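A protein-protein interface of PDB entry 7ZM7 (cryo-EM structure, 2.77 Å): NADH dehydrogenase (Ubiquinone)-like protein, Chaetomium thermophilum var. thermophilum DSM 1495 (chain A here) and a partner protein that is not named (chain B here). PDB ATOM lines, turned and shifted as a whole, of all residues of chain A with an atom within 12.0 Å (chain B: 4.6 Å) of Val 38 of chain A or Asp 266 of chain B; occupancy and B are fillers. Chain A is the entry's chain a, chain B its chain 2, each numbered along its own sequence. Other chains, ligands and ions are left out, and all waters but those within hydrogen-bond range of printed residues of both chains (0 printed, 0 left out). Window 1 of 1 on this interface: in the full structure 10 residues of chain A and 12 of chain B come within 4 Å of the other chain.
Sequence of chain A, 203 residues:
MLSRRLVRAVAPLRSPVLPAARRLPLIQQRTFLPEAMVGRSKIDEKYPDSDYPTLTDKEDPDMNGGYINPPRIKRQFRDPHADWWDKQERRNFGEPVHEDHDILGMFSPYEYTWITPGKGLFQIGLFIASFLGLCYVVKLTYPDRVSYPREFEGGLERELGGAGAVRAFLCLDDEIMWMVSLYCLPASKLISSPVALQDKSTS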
ATOM      1  N   PHE A  32     -17.517 -13.073  21.946  1.00  0.00           N
ATOM      2  CA  PHE A  32     -18.892 -13.551  22.228  1.00  0.00           C
ATOM      3  C   PHE A  32     -19.443 -12.824  23.455  1.00  0.00           C
ATOM      4  O   PHE A  32     -20.613 -13.045  23.808  1.00  0.00           O
ATOM      5  CB  PHE A  32     -18.904 -15.058  22.497  1.00  0.00           C
ATOM      6  CG  PHE A  32     -18.858 -15.933  21.273  1.00  0.00           C
ATOM      7  CD1 PHE A  32     -19.588 -15.608  20.143  1.00  0.00           C
ATOM      8  CD2 PHE A  32     -18.102 -17.092  21.263  1.00  0.00           C
ATOM      9  CE1 PHE A  32     -19.557 -16.421  19.022  1.00  0.00           C
ATOM     10  CE2 PHE A  32     -18.069 -17.903  20.141  1.00  0.00           C
ATOM     11  CZ  PHE A  32     -18.798 -17.566  19.025  1.00  0.00           C
ATOM     12  N   LEU A  33     -18.614 -12.000  24.096  1.00  0.00           N
ATOM     13  CA  LEU A  33     -19.057 -11.343  25.348  1.00  0.00           C
ATOM     14  C   LEU A  33     -19.586  -9.916  25.106  1.00  0.00           C
ATOM     15  O   LEU A  33     -19.119  -9.280  24.152  1.00  0.00           O
ATOM     16  CB  LEU A  33     -17.943 -11.394  26.394  1.00  0.00           C
ATOM     17  CG  LEU A  33     -17.848 -12.709  27.166  1.00  0.00           C
ATOM     18  CD1 LEU A  33     -16.689 -12.679  28.147  1.00  0.00           C
ATOM     19  CD2 LEU A  33     -19.149 -13.001  27.896  1.00  0.00           C
ATOM     20  N   PRO A  34     -20.543  -9.386  25.915  1.00  0.00           N
ATOM     21  CA  PRO A  34     -21.052  -8.030  25.717  1.00  0.00           C
ATOM     22  C   PRO A  34     -19.966  -6.980  25.853  1.00  0.00           C
ATOM     23  O   PRO A  34     -19.014  -7.124  26.618  1.00  0.00           O
ATOM     24  CB  PRO A  34     -22.101  -7.885  26.820  1.00  0.00           C
ATOM     25  CG  PRO A  34     -22.438  -9.259  27.181  1.00  0.00           C
ATOM     26  CD  PRO A  34     -21.227 -10.060  27.025  1.00  0.00           C
ATOM     27  N   GLU A  35     -20.137  -5.903  25.092  1.00  0.00           N
ATOM     28  CA  GLU A  35     -19.172  -4.815  25.026  1.00  0.00           C
ATOM     29  C   GLU A  35     -19.050  -4.077  26.350  1.00  0.00           C
ATOM     30  O   GLU A  35     -18.030  -3.434  26.598  1.00  0.00           O
ATOM     31  CB  GLU A  35     -19.589  -3.874  23.895  1.00  0.00           C
ATOM     32  CG  GLU A  35     -18.690  -2.682  23.614  1.00  0.00           C
ATOM     33  CD  GLU A  35     -17.318  -3.078  23.114  1.00  0.00           C
ATOM     34  OE1 GLU A  35     -17.188  -4.174  22.531  1.00  0.00           O
ATOM     35  OE2 GLU A  35     -16.375  -2.275  23.276  1.00  0.00           O
ATOM     36  N   ALA A  36     -20.060  -4.161  27.209  1.00  0.00           N
ATOM     37  CA  ALA A  36     -19.991  -3.495  28.498  1.00  0.00           C
ATOM     38  C   ALA A  36     -18.988  -4.159  29.420  1.00  0.00           C
ATOM     39  O   ALA A  36     -18.503  -3.533  30.364  1.00  0.00           O
ATOM     40  CB  ALA A  36     -21.367  -3.491  29.141  1.00  0.00           C
ATOM     41  N   MET A  37     -18.657  -5.416  29.151  1.00  0.00           N
ATOM     42  CA  MET A  37     -17.929  -6.277  30.063  1.00  0.00           C
ATOM     43  C   MET A  37     -16.468  -6.440  29.689  1.00  0.00           C
ATOM     44  O   MET A  37     -15.606  -6.449  30.568  1.00  0.00           O
ATOM     45  CB  MET A  37     -18.605  -7.647  30.099  1.00  0.00           C
ATOM     46  CG  MET A  37     -19.987  -7.603  30.705  1.00  0.00           C
ATOM     47  SD  MET A  37     -20.886  -9.151  30.709  1.00  0.00           S
ATOM     48  CE  MET A  37     -20.003 -10.112  31.920  1.00  0.00           C
ATOM     49  N   VAL A  38     -16.170  -6.592  28.402  1.00  0.00           N
ATOM     50  CA  VAL A  38     -14.803  -6.711  27.915  1.00  0.00           C
ATOM     51  C   VAL A  38     -14.401  -5.536  27.047  1.00  0.00           C
ATOM     52  O   VAL A  38     -13.221  -5.402  26.713  1.00  0.00           O
ATOM     53  CB  VAL A  38     -14.590  -8.031  27.142  1.00  0.00           C
ATOM     54  CG1 VAL A  38     -15.033  -9.214  27.964  1.00  0.00           C
ATOM     55  CG2 VAL A  38     -15.316  -7.994  25.798  1.00  0.00           C
ATOM     56  N   GLY A  39     -15.343  -4.666  26.697  1.00  0.00           N
ATOM     57  CA  GLY A  39     -15.058  -3.633  25.719  1.00  0.00           C
ATOM     58  C   GLY A  39     -14.026  -2.635  26.212  1.00  0.00           C
ATOM     59  O   GLY A  39     -14.006  -2.252  27.381  1.00  0.00           O
ATOM     60  N   ARG A  40     -13.155  -2.172  25.314  1.00  0.00           N
ATOM     61  CA  ARG A  40     -12.112  -1.179  25.691  1.00  0.00           C
ATOM     62  C   ARG A  40     -12.773   0.171  25.993  1.00  0.00           C
ATOM     63  O   ARG A  40     -12.116   1.022  26.622  1.00  0.00           O
ATOM     64  CB  ARG A  40     -11.093  -1.093  24.546  1.00  0.00           C
ATOM     65  CG  ARG A  40     -10.109   0.068  24.611  1.00  0.00           C
ATOM     66  CD  ARG A  40      -9.054  -0.015  25.701  1.00  0.00           C
ATOM     67  NE  ARG A  40      -8.419   1.278  25.923  1.00  0.00           N
ATOM     68  CZ  ARG A  40      -7.334   1.717  25.292  1.00  0.00           C
ATOM     69  NH1 ARG A  40      -6.848   2.913  25.572  1.00  0.00           N
ATOM     70  NH2 ARG A  40      -6.736   0.960  24.390  1.00  0.00           N
ATOM     71  N   SER A  41     -14.052   0.336  25.644  1.00  0.00           N
ATOM     72  CA  SER A  41     -14.672   1.645  25.774  1.00  0.00           C
ATOM     73  C   SER A  41     -14.864   2.040  27.233  1.00  0.00           C
ATOM     74  O   SER A  41     -14.513   3.155  27.631  1.00  0.00           O
ATOM     75  CB  SER A  41     -16.007   1.645  25.032  1.00  0.00           C
ATOM     76  OG  SER A  41     -15.850   1.107  23.730  1.00  0.00           O
ATOM     77  N   LYS A  42     -15.432   1.154  28.045  1.00  0.00           N
ATOM     78  CA  LYS A  42     -15.686   1.536  29.424  1.00  0.00           C
ATOM     79  C   LYS A  42     -14.431   1.656  30.253  1.00  0.00           C
ATOM     80  O   LYS A  42     -14.507   2.187  31.362  1.00  0.00           O
ATOM     81  CB  LYS A  42     -16.671   0.584  30.104  1.00  0.00           C
ATOM     82  CG  LYS A  42     -18.025   0.683  29.516  1.00  0.00           C
ATOM     83  CD  LYS A  42     -19.015  -0.220  30.163  1.00  0.00           C
ATOM     84  CE  LYS A  42     -20.376   0.045  29.549  1.00  0.00           C
ATOM     85  NZ  LYS A  42     -20.455  -0.341  28.112  1.00  0.00           N
ATOM     86  N   ILE A  43     -13.293   1.184  29.766  1.00  0.00           N
ATOM     87  CA  ILE A  43     -12.047   1.587  30.398  1.00  0.00           C
ATOM     88  C   ILE A  43     -11.753   3.048  30.098  1.00  0.00           C
ATOM     89  O   ILE A  43     -11.401   3.818  30.995  1.00  0.00           O
ATOM     90  CB  ILE A  43     -10.907   0.644  29.993  1.00  0.00           C
ATOM     91  CG1 ILE A  43     -11.206  -0.766  30.502  1.00  0.00           C
ATOM     92  CG2 ILE A  43      -9.619   1.098  30.577  1.00  0.00           C
ATOM     93  CD1 ILE A  43     -11.994  -1.631  29.589  1.00  0.00           C
ATOM     94  N   ASP A  44     -11.966   3.475  28.853  1.00  0.00           N
ATOM     95  CA  ASP A  44     -11.843   4.881  28.496  1.00  0.00           C
ATOM     96  C   ASP A  44     -12.900   5.759  29.151  1.00  0.00           C
ATOM     97  O   ASP A  44     -12.784   6.986  29.095  1.00  0.00           O
ATOM     98  CB  ASP A  44     -11.931   5.037  26.989  1.00  0.00           C
ATOM     99  CG  ASP A  44     -10.806   4.344  26.279  1.00  0.00           C
ATOM    100  OD1 ASP A  44     -10.060   3.620  26.961  1.00  0.00           O
ATOM    101  OD2 ASP A  44     -10.663   4.520  25.049  1.00  0.00           O
ATOM    102  N   GLU A  45     -13.942   5.177  29.729  1.00  0.00           N
ATOM    103  CA  GLU A  45     -14.908   5.952  30.491  1.00  0.00           C
ATOM    104  C   GLU A  45     -14.598   5.912  31.980  1.00  0.00           C
ATOM    105  O   GLU A  45     -14.904   6.857  32.707  1.00  0.00           O
ATOM    106  CB  GLU A  45     -16.322   5.431  30.222  1.00  0.00           C
ATOM    107  CG  GLU A  45     -17.433   6.215  30.905  1.00  0.00           C
ATOM    108  CD  GLU A  45     -17.595   7.610  30.345  1.00  0.00           C
ATOM    109  OE1 GLU A  45     -17.279   7.811  29.155  1.00  0.00           O
ATOM    110  OE2 GLU A  45     -18.034   8.507  31.095  1.00  0.00           O
ATOM    111  N   LYS A  46     -13.982   4.830  32.442  1.00  0.00           N
ATOM    112  CA  LYS A  46     -13.576   4.714  33.832  1.00  0.00           C
ATOM    113  C   LYS A  46     -12.185   5.282  34.057  1.00  0.00           C
ATOM    114  O   LYS A  46     -11.894   5.796  35.142  1.00  0.00           O
ATOM    115  CB  LYS A  46     -13.618   3.246  34.260  1.00  0.00           C
ATOM    116  CG  LYS A  46     -14.998   2.704  34.531  1.00  0.00           C
ATOM    117  CD  LYS A  46     -15.740   3.535  35.571  1.00  0.00           C
ATOM    118  CE  LYS A  46     -16.765   2.697  36.335  1.00  0.00           C
ATOM    119  NZ  LYS A  46     -17.368   1.614  35.518  1.00  0.00           N
ATOM    120  N   TYR A  47     -11.314   5.179  33.061  1.00  0.00           N
ATOM    121  CA  TYR A  47      -9.942   5.666  33.146  1.00  0.00           C
ATOM    122  C   TYR A  47      -9.641   6.469  31.893  1.00  0.00           C
ATOM    123  O   TYR A  47      -8.771   6.097  31.098  1.00  0.00           O
ATOM    124  CB  TYR A  47      -8.956   4.508  33.300  1.00  0.00           C
ATOM    125  CG  TYR A  47      -9.102   3.755  34.597  1.00  0.00           C
ATOM    126  CD1 TYR A  47      -8.507   4.217  35.749  1.00  0.00           C
ATOM    127  CD2 TYR A  47      -9.841   2.578  34.665  1.00  0.00           C
ATOM    128  CE1 TYR A  47      -8.646   3.541  36.930  1.00  0.00           C
ATOM    129  CE2 TYR A  47      -9.978   1.891  35.841  1.00  0.00           C
ATOM    130  CZ  TYR A  47      -9.380   2.377  36.974  1.00  0.00           C
ATOM    131  OH  TYR A  47      -9.508   1.705  38.167  1.00  0.00           O
ATOM    132  N   PHE B 262      -5.462 -15.274  28.663  1.00  0.00           N
ATOM    133  CA  PHE B 262      -6.544 -14.347  28.230  1.00  0.00           C
ATOM    134  C   PHE B 262      -7.915 -14.964  28.529  1.00  0.00           C
ATOM    135  O   PHE B 262      -8.879 -14.207  28.746  1.00  0.00           O
ATOM    136  CB  PHE B 262      -6.372 -13.957  26.759  1.00  0.00           C
ATOM    137  CG  PHE B 262      -5.097 -13.229  26.418  1.00  0.00           C
ATOM    138  CD1 PHE B 262      -3.958 -13.927  26.054  1.00  0.00           C
ATOM    139  CD2 PHE B 262      -5.040 -11.845  26.437  1.00  0.00           C
ATOM    140  CE1 PHE B 262      -2.790 -13.259  25.729  1.00  0.00           C
ATOM    141  CE2 PHE B 262      -3.869 -11.177  26.115  1.00  0.00           C
ATOM    142  CZ  PHE B 262      -2.747 -11.885  25.760  1.00  0.00           C
ATOM    143  N   TRP B 263      -7.986 -16.285  28.648  1.00  0.00           N
ATOM    144  CA  TRP B 263      -9.294 -16.963  28.851  1.00  0.00           C
ATOM    145  C   TRP B 263      -9.859 -16.725  30.253  1.00  0.00           C
ATOM    146  O   TRP B 263     -11.071 -16.497  30.347  1.00  0.00           O
ATOM    147  CB  TRP B 263      -9.154 -18.463  28.568  1.00  0.00           C
ATOM    148  CG  TRP B 263      -8.378 -19.196  29.619  1.00  0.00           C
ATOM    149  CD1 TRP B 263      -7.022 -19.312  29.710  1.00  0.00           C
ATOM    150  CD2 TRP B 263      -8.913 -19.897  30.757  1.00  0.00           C
ATOM    151  NE1 TRP B 263      -6.679 -20.051  30.808  1.00  0.00           N
ATOM    152  CE2 TRP B 263      -7.817 -20.418  31.474  1.00  0.00           C
ATOM    153  CE3 TRP B 263     -10.205 -20.130  31.239  1.00  0.00           C
ATOM    154  CZ2 TRP B 263      -7.978 -21.165  32.639  1.00  0.00           C
ATOM    155  CZ3 TRP B 263     -10.362 -20.857  32.397  1.00  0.00           C
ATOM    156  CH2 TRP B 263      -9.263 -21.373  33.083  1.00  0.00           C
ATOM    157  N   SER B 264      -9.025 -16.739  31.294  1.00  0.00           N
ATOM    158  CA  SER B 264      -9.554 -16.686  32.684  1.00  0.00           C
ATOM    159  C   SER B 264     -10.348 -15.418  33.013  1.00  0.00           C
ATOM    160  O   SER B 264     -11.437 -15.577  33.578  1.00  0.00           O
ATOM    161  CB  SER B 264      -8.466 -16.913  33.688  1.00  0.00           C
ATOM    162  OG  SER B 264      -8.407 -18.278  34.063  1.00  0.00           O
ATOM    163  N   PRO B 265      -9.909 -14.178  32.701  1.00  0.00           N
ATOM    164  CA  PRO B 265     -10.693 -13.007  33.071  1.00  0.00           C
ATOM    165  C   PRO B 265     -12.090 -13.087  32.450  1.00  0.00           C
ATOM    166  O   PRO B 265     -13.035 -12.749  33.131  1.00  0.00           O
ATOM    167  CB  PRO B 265      -9.883 -11.836  32.514  1.00  0.00           C
ATOM    168  CG  PRO B 265      -8.469 -12.359  32.503  1.00  0.00           C
ATOM    169  CD  PRO B 265      -8.622 -13.809  32.106  1.00  0.00           C
ATOM    170  N   ASP B 266     -12.186 -13.571  31.209  1.00  0.00           N
ATOM    171  CA  ASP B 266     -13.470 -13.611  30.521  1.00  0.00           C
ATOM    172  C   ASP B 266     -14.374 -14.698  31.070  1.00  0.00           C
ATOM    173  O   ASP B 266     -15.565 -14.467  31.267  1.00  0.00           O
ATOM    174  CB  ASP B 266     -13.245 -13.794  29.025  1.00  0.00           C
ATOM    175  CG  ASP B 266     -12.613 -12.590  28.404  1.00  0.00           C
ATOM    176  OD1 ASP B 266     -11.944 -11.852  29.140  1.00  0.00           O
ATOM    177  OD2 ASP B 266     -12.787 -12.359  27.199  1.00  0.00           O
ATOM    178  N   VAL B 267     -13.832 -15.878  31.327  1.00  0.00           N
ATOM    179  CA  VAL B 267     -14.673 -17.012  31.796  1.00  0.00           C
ATOM    180  C   VAL B 267     -15.077 -16.749  33.249  1.00  0.00           C
ATOM    181  O   VAL B 267     -16.243 -16.976  33.586  1.00  0.00           O
ATOM    182  CB  VAL B 267     -13.985 -18.372  31.575  1.00  0.00           C
ATOM    183  CG1 VAL B 267     -14.706 -19.514  32.277  1.00  0.00           C
ATOM    184  CG2 VAL B 267     -13.808 -18.679  30.099  1.00  0.00           C
ATOM    185  N   TYR B 268     -14.153 -16.255  34.068  1.00  0.00           N
ATOM    186  CA  TYR B 268     -14.435 -16.060  35.513  1.00  0.00           C
ATOM    187  C   TYR B 268     -15.473 -14.959  35.754  1.00  0.00           C
ATOM    188  O   TYR B 268     -16.122 -15.006  36.792  1.00  0.00           O
ATOM    189  CB  TYR B 268     -13.144 -15.920  36.326  1.00  0.00           C
ATOM    190  CG  TYR B 268     -12.267 -17.143  36.388  1.00  0.00           C
ATOM    191  CD1 TYR B 268     -12.747 -18.395  36.039  1.00  0.00           C
ATOM    192  CD2 TYR B 268     -10.950 -17.048  36.809  1.00  0.00           C
ATOM    193  CE1 TYR B 268     -11.939 -19.517  36.092  1.00  0.00           C
ATOM    194  CE2 TYR B 268     -10.131 -18.162  36.871  1.00  0.00           C
ATOM    195  CZ  TYR B 268     -10.626 -19.401  36.509  1.00  0.00           C
ATOM    196  OH  TYR B 268      -9.827 -20.506  36.570  1.00  0.00           O
ATOM    197  N   ASP B 269     -15.640 -14.030  34.819  1.00  0.00           N
ATOM    198  CA  ASP B 269     -16.577 -12.890  34.970  1.00  0.00           C
ATOM    199  C   ASP B 269     -17.935 -13.291  34.409  1.00  0.00           C
ATOM    200  O   ASP B 269     -18.936 -12.806  34.937  1.00  0.00           O
ATOM    201  CB  ASP B 269     -16.095 -11.714  34.127  1.00  0.00           C
ATOM    202  CG  ASP B 269     -16.709 -10.367  34.464  1.00  0.00           C
ATOM    203  OD1 ASP B 269     -16.907 -10.093  35.662  1.00  0.00           O
ATOM    204  OD2 ASP B 269     -16.968  -9.598  33.522  1.00  0.00           O
ATOM    205  N   ALA B 270     -17.970 -14.172  33.414  1.00  0.00           N
ATOM    206  CA  ALA B 270     -19.215 -14.535  32.756  1.00  0.00           C
ATOM    207  C   ALA B 270     -20.029 -15.565  33.529  1.00  0.00           C
ATOM    208  O   ALA B 270     -21.259 -15.524  33.497  1.00  0.00           O
ATOM    209  CB  ALA B 270     -18.911 -15.051  31.349  1.00  0.00           C
ATOM    210  N   ARG B 338     -13.188  -9.761  37.117  1.00  0.00           N
ATOM    211  CA  ARG B 338     -12.021  -9.612  36.255  1.00  0.00           C
ATOM    212  C   ARG B 338     -10.799  -9.183  37.055  1.00  0.00           C
ATOM    213  O   ARG B 338      -9.676  -9.579  36.742  1.00  0.00           O
ATOM    214  CB  ARG B 338     -12.295  -8.595  35.152  1.00  0.00           C
ATOM    215  CG  ARG B 338     -13.405  -8.949  34.231  1.00  0.00           C
ATOM    216  CD  ARG B 338     -13.395  -8.074  33.025  1.00  0.00           C
ATOM    217  NE  ARG B 338     -12.150  -8.189  32.282  1.00  0.00           N
ATOM    218  CZ  ARG B 338     -11.941  -9.071  31.313  1.00  0.00           C
ATOM    219  NH1 ARG B 338     -12.901  -9.922  30.965  1.00  0.00           N
ATOM    220  NH2 ARG B 338     -10.775  -9.099  30.693  1.00  0.00           N
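Among the printed residues, pairs that only touch across the chains: Leu 33 of chain A with Asp 266 of chain B (3.7 Å), Met 37 of chain A with Asp 269 of chain B (3.5 Å), Met 37 of chain A with Arg 338 of chain B (3.7 Å), Val 38 of chain A with Asp 266 of chain B (3.9 Å) and Val 38 of chain A with Arg 338 of chain B (3.7 Å).
Printed residues of chain B within 4 Å of Leu 33 of chain A: Asp 266 (3.7 Å). Printed residues of chain B within 4 Å of Met 37 of chain A: Asp 269 and Arg 338. Val 38 of chain A touches just these residues of chain B: Asp 266 (3.9 Å) and Arg 338 (3.7 Å). No residue of chain A comes within 4 Å of Ser 264 of chain B. No residue of chain A comes within 4 Å of Pro 265 of chain B. No residue of chain A comes within 4 Å of Val 267 of chain B. Of chain A, only Met 37 comes within 4 Å of Asp 269 of chain B. No residue of chain A comes within 4 Å of Ala 270 of chain B. The nearest residue of chain A that does not touch Asp 266 of chain B is Met 37 of chain A (6.3 Å).
The guanidinium group (NH1) of Arg 338 of chain B is in salt-bridge range of the side-chain carboxylate (OD1) of Asp 266 of chain B (2.8 Å).
Printed residues of chain B that touch a printed residue of chain A: Asp 266, Asp 269 and Arg 338. Hydrophobic or aromatic side chains of chain A that line the printed part of chain B: Leu 33, Met 37 and Val 38. Among the printed residues, no Asp or Glu carboxylate lies within 4 Å of a Lys or Arg side-chain nitrogen of the other chain.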
